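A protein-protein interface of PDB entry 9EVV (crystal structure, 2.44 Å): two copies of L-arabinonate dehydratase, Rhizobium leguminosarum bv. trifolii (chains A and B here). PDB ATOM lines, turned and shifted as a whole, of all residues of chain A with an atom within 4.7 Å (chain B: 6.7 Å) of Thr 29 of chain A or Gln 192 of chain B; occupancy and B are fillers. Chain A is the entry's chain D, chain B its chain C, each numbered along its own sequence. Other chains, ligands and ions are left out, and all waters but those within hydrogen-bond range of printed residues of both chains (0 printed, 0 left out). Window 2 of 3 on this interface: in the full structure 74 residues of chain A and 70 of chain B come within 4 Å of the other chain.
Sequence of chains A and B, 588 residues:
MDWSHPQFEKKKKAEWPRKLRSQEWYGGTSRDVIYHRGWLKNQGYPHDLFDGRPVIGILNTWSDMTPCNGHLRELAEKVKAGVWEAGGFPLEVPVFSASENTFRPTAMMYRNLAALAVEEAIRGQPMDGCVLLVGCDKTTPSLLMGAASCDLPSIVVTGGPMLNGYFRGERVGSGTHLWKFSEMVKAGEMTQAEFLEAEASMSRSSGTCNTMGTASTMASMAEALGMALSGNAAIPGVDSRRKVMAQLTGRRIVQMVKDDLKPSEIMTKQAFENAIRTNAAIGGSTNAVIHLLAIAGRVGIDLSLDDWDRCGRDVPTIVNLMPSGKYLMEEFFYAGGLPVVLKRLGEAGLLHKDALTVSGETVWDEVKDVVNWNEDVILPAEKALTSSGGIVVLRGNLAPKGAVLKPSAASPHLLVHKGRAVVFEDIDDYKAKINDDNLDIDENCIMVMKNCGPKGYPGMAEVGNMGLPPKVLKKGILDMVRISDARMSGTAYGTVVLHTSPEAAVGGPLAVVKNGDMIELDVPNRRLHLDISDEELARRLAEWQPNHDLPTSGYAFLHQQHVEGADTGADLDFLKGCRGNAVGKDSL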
ATOM      1  N   GLY A  27      -0.068  -4.518  21.791  1.00  0.00           N
ATOM      2  CA  GLY A  27       0.752  -4.325  22.979  1.00  0.00           C
ATOM      3  C   GLY A  27       1.821  -3.266  22.756  1.00  0.00           C
ATOM      4  O   GLY A  27       2.382  -3.150  21.664  1.00  0.00           O
ATOM      5  N   GLY A  28       2.088  -2.489  23.795  1.00  0.00           N
ATOM      6  CA  GLY A  28       3.203  -1.567  23.769  1.00  0.00           C
ATOM      7  C   GLY A  28       2.835  -0.155  23.362  1.00  0.00           C
ATOM      8  O   GLY A  28       1.693   0.289  23.475  1.00  0.00           O
ATOM      9  N   THR A  29       3.850   0.565  22.857  1.00  0.00           N
ATOM     10  CA  THR A  29       3.783   2.014  22.708  1.00  0.00           C
ATOM     11  C   THR A  29       4.239   2.559  21.357  1.00  0.00           C
ATOM     12  O   THR A  29       4.158   3.776  21.145  1.00  0.00           O
ATOM     13  CB  THR A  29       4.622   2.676  23.804  1.00  0.00           C
ATOM     14  OG1 THR A  29       5.901   2.043  23.834  1.00  0.00           O
ATOM     15  CG2 THR A  29       3.962   2.513  25.156  1.00  0.00           C
ATOM     16  N   SER A  30       4.716   1.720  20.440  1.00  0.00           N
ATOM     17  CA  SER A  30       5.232   2.240  19.183  1.00  0.00           C
ATOM     18  C   SER A  30       4.118   2.896  18.375  1.00  0.00           C
ATOM     19  O   SER A  30       2.944   2.548  18.499  1.00  0.00           O
ATOM     20  CB  SER A  30       5.885   1.119  18.371  1.00  0.00           C
ATOM     21  OG  SER A  30       4.958   0.120  17.995  1.00  0.00           O
ATOM     22  N   ARG A  31       4.493   3.863  17.539  1.00  0.00           N
ATOM     23  CA  ARG A  31       3.517   4.432  16.612  1.00  0.00           C
ATOM     24  C   ARG A  31       2.727   3.348  15.875  1.00  0.00           C
ATOM     25  O   ARG A  31       1.549   3.553  15.569  1.00  0.00           O
ATOM     26  CB  ARG A  31       4.200   5.356  15.596  1.00  0.00           C
ATOM     27  CG  ARG A  31       4.884   4.606  14.481  1.00  0.00           C
ATOM     28  CD  ARG A  31       4.540   5.168  13.123  1.00  0.00           C
ATOM     29  NE  ARG A  31       5.114   4.334  12.075  1.00  0.00           N
ATOM     30  CZ  ARG A  31       6.014   4.754  11.200  1.00  0.00           C
ATOM     31  NH1 ARG A  31       6.439   6.006  11.197  1.00  0.00           N
ATOM     32  NH2 ARG A  31       6.504   3.896  10.310  1.00  0.00           N
ATOM     33  N   ILE A  34       0.006   2.335  18.385  1.00  0.00           N
ATOM     34  CA  ILE A  34      -0.933   3.450  18.499  1.00  0.00           C
ATOM     35  C   ILE A  34      -1.904   3.430  17.325  1.00  0.00           C
ATOM     36  O   ILE A  34      -3.103   3.708  17.478  1.00  0.00           O
ATOM     37  CB  ILE A  34      -0.187   4.798  18.570  1.00  0.00           C
ATOM     38  CG1 ILE A  34       0.718   4.892  19.792  1.00  0.00           C
ATOM     39  CG2 ILE A  34      -1.178   5.951  18.634  1.00  0.00           C
ATOM     40  CD1 ILE A  34       1.333   6.287  19.965  1.00  0.00           C
ATOM     41  N   PHE B 181       3.899  13.214  14.202  1.00  0.00           N
ATOM     42  CA  PHE B 181       4.226  12.955  15.604  1.00  0.00           C
ATOM     43  C   PHE B 181       5.408  11.997  15.750  1.00  0.00           C
ATOM     44  O   PHE B 181       6.234  12.165  16.658  1.00  0.00           O
ATOM     45  CB  PHE B 181       2.996  12.420  16.327  1.00  0.00           C
ATOM     46  CG  PHE B 181       1.943  13.459  16.552  1.00  0.00           C
ATOM     47  CD1 PHE B 181       2.160  14.772  16.146  1.00  0.00           C
ATOM     48  CD2 PHE B 181       0.719  13.125  17.144  1.00  0.00           C
ATOM     49  CE1 PHE B 181       1.185  15.748  16.349  1.00  0.00           C
ATOM     50  CE2 PHE B 181      -0.268  14.095  17.352  1.00  0.00           C
ATOM     51  CZ  PHE B 181      -0.036  15.409  16.955  1.00  0.00           C
ATOM     52  N   SER B 182       5.515  10.987  14.874  1.00  0.00           N
ATOM     53  CA  SER B 182       6.651  10.072  14.987  1.00  0.00           C
ATOM     54  C   SER B 182       7.936  10.685  14.431  1.00  0.00           C
ATOM     55  O   SER B 182       9.027  10.347  14.906  1.00  0.00           O
ATOM     56  CB  SER B 182       6.354   8.725  14.310  1.00  0.00           C
ATOM     57  OG  SER B 182       5.525   8.859  13.174  1.00  0.00           O
ATOM     58  N   VAL B 185       9.177  12.900  17.361  1.00  0.00           N
ATOM     59  CA  VAL B 185       9.837  12.158  18.432  1.00  0.00           C
ATOM     60  C   VAL B 185      11.267  11.808  18.027  1.00  0.00           C
ATOM     61  O   VAL B 185      12.188  11.842  18.852  1.00  0.00           O
ATOM     62  CB  VAL B 185       9.015  10.903  18.805  1.00  0.00           C
ATOM     63  CG1 VAL B 185       9.821   9.965  19.702  1.00  0.00           C
ATOM     64  CG2 VAL B 185       7.692  11.290  19.486  1.00  0.00           C
ATOM     65  N   MET B 190       9.115  16.178  20.631  1.00  0.00           N
ATOM     66  CA  MET B 190       7.982  15.601  21.349  1.00  0.00           C
ATOM     67  C   MET B 190       8.332  14.172  21.751  1.00  0.00           C
ATOM     68  O   MET B 190       9.073  13.484  21.043  1.00  0.00           O
ATOM     69  CB  MET B 190       6.712  15.648  20.485  1.00  0.00           C
ATOM     70  CG  MET B 190       5.622  14.643  20.818  1.00  0.00           C
ATOM     71  SD  MET B 190       4.413  14.563  19.472  1.00  0.00           S
ATOM     72  CE  MET B 190       2.898  14.377  20.416  1.00  0.00           C
ATOM     73  N   THR B 191       7.803  13.738  22.897  1.00  0.00           N
ATOM     74  CA  THR B 191       8.112  12.432  23.476  1.00  0.00           C
ATOM     75  C   THR B 191       7.061  11.382  23.116  1.00  0.00           C
ATOM     76  O   THR B 191       5.890  11.697  22.898  1.00  0.00           O
ATOM     77  CB  THR B 191       8.231  12.533  25.002  1.00  0.00           C
ATOM     78  OG1 THR B 191       6.933  12.371  25.612  1.00  0.00           O
ATOM     79  CG2 THR B 191       8.844  13.881  25.405  1.00  0.00           C
ATOM     80  N   GLN B 192       7.493  10.121  23.063  1.00  0.00           N
ATOM     81  CA  GLN B 192       6.535   9.041  22.871  1.00  0.00           C
ATOM     82  C   GLN B 192       5.447   9.073  23.934  1.00  0.00           C
ATOM     83  O   GLN B 192       4.313   8.661  23.671  1.00  0.00           O
ATOM     84  CB  GLN B 192       7.233   7.685  22.888  1.00  0.00           C
ATOM     85  CG  GLN B 192       6.482   6.581  22.151  1.00  0.00           C
ATOM     86  CD  GLN B 192       6.311   6.892  20.674  1.00  0.00           C
ATOM     87  OE1 GLN B 192       6.993   7.758  20.132  1.00  0.00           O
ATOM     88  NE2 GLN B 192       5.414   6.171  20.014  1.00  0.00           N
ATOM     89  N   ALA B 193       5.777   9.552  25.135  1.00  0.00           N
ATOM     90  CA  ALA B 193       4.771   9.740  26.175  1.00  0.00           C
ATOM     91  C   ALA B 193       3.638  10.647  25.700  1.00  0.00           C
ATOM     92  O   ALA B 193       2.457  10.283  25.792  1.00  0.00           O
ATOM     93  CB  ALA B 193       5.419  10.310  27.437  1.00  0.00           C
ATOM     94  N   GLU B 194       3.972  11.839  25.193  1.00  0.00           N
ATOM     95  CA  GLU B 194       2.917  12.747  24.745  1.00  0.00           C
ATOM     96  C   GLU B 194       2.212  12.222  23.499  1.00  0.00           C
ATOM     97  O   GLU B 194       1.019  12.485  23.314  1.00  0.00           O
ATOM     98  CB  GLU B 194       3.478  14.143  24.482  1.00  0.00           C
ATOM     99  CG  GLU B 194       4.563  14.585  25.451  1.00  0.00           C
ATOM    100  CD  GLU B 194       5.458  15.656  24.845  1.00  0.00           C
ATOM    101  OE1 GLU B 194       4.983  16.808  24.727  1.00  0.00           O
ATOM    102  OE2 GLU B 194       6.615  15.351  24.457  1.00  0.00           O
ATOM    103  N   PHE B 195       2.932  11.492  22.637  1.00  0.00           N
ATOM    104  CA  PHE B 195       2.317  10.812  21.498  1.00  0.00           C
ATOM    105  C   PHE B 195       1.238   9.818  21.954  1.00  0.00           C
ATOM    106  O   PHE B 195       0.191   9.687  21.304  1.00  0.00           O
ATOM    107  CB  PHE B 195       3.421  10.121  20.680  1.00  0.00           C
ATOM    108  CG  PHE B 195       3.024   9.731  19.270  1.00  0.00           C
ATOM    109  CD1 PHE B 195       1.757   9.997  18.775  1.00  0.00           C
ATOM    110  CD2 PHE B 195       3.939   9.086  18.440  1.00  0.00           C
ATOM    111  CE1 PHE B 195       1.405   9.626  17.478  1.00  0.00           C
ATOM    112  CE2 PHE B 195       3.595   8.709  17.143  1.00  0.00           C
ATOM    113  CZ  PHE B 195       2.325   8.985  16.662  1.00  0.00           C
ATOM    114  N   LEU B 196       1.455   9.140  23.092  1.00  0.00           N
ATOM    115  CA  LEU B 196       0.479   8.186  23.618  1.00  0.00           C
ATOM    116  C   LEU B 196      -0.785   8.850  24.161  1.00  0.00           C
ATOM    117  O   LEU B 196      -1.826   8.186  24.258  1.00  0.00           O
ATOM    118  CB  LEU B 196       1.122   7.333  24.711  1.00  0.00           C
ATOM    119  CG  LEU B 196       1.463   5.889  24.336  1.00  0.00           C
ATOM    120  CD1 LEU B 196       0.198   5.062  24.236  1.00  0.00           C
ATOM    121  CD2 LEU B 196       2.256   5.820  23.033  1.00  0.00           C
ATOM    122  N   GLU B 197      -0.731  10.128  24.529  1.00  0.00           N
ATOM    123  CA  GLU B 197      -1.944  10.803  24.969  1.00  0.00           C
ATOM    124  C   GLU B 197      -2.800  11.292  23.810  1.00  0.00           C
ATOM    125  O   GLU B 197      -3.967  11.639  24.020  1.00  0.00           O
ATOM    126  CB  GLU B 197      -1.597  11.981  25.879  1.00  0.00           C
ATOM    127  CG  GLU B 197      -1.200  11.568  27.279  1.00  0.00           C
ATOM    128  CD  GLU B 197       0.129  12.158  27.650  1.00  0.00           C
ATOM    129  OE1 GLU B 197       0.571  13.061  26.909  1.00  0.00           O
ATOM    130  OE2 GLU B 197       0.727  11.728  28.660  1.00  0.00           O
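O of Thr 29 of chain A is in hydrogen-bond range of NE2 of Gln 192 of chain B.
Leu 196 of chain B touches Thr 29 of chain A (CD2 to O, 3.4 Å). C of Ser 30 of chain A touches NE2 of Gln 192 of chain B, 3.9 Å away. Arg 31 of chain A touches Ser 182 of chain B. Arg 31 of chain A touches Gln 192 of chain B. Phe 195 of chain B touches Arg 31 of chain A (CE2 to CB, 3.7 Å). Ile 34 of chain A touches Phe 195 of chain B (CD1 to O, 3.8 Å). CD1 of Ile 34 of chain A touches CD2 of Leu 196 of chain B (3.2 Å).
Of chain B, only Gln 192 (2.9 Å) and Leu 196 (3.4 Å) come within 4 Å of Thr 29 of chain A. Printed residues of chain B within 4 Å of Ile 34 of chain A: Phe 195 (3.8 Å) and Leu 196 (3.2 Å). Printed residues of chain A within 4 Å of Ser 182 of chain B: Arg 31 (3.6 Å). Printed residues of chain B within 4 Å of Ser 30 of chain A: Gln 192 (3.9 Å). Thr 191 of chain B touches none of the printed residues of chain A. The nearest residue of chain A that does not touch Gln 192 of chain B is Ile 34 of chain A (4.1 Å). The nearest printed residue of chain A that does not touch Phe 195 of chain B is Thr 29 of chain A (6.0 Å).
Of the 11 printed residues of chain B, 4 touch a printed residue of chain A. Of the 6 printed residues of chain A, 4 touch a printed residue of chain B. Printed residues of chain A that touch a printed residue of chain B: Thr 29, Ser 30, Arg 31 and Ile 34. Hydrophobic or aromatic side chains of chain A within 4 Å of the printed part of chain B: Ile 34. Among the printed residues, no Asp or Glu carboxylate lies within 4 Å of a Lys or Arg side-chain nitrogen of the other chain.
No position is printed for both chains. Of the 8 pairs that touch across the chains among the printed residues, none has its exchanged pair printed and touching as well.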
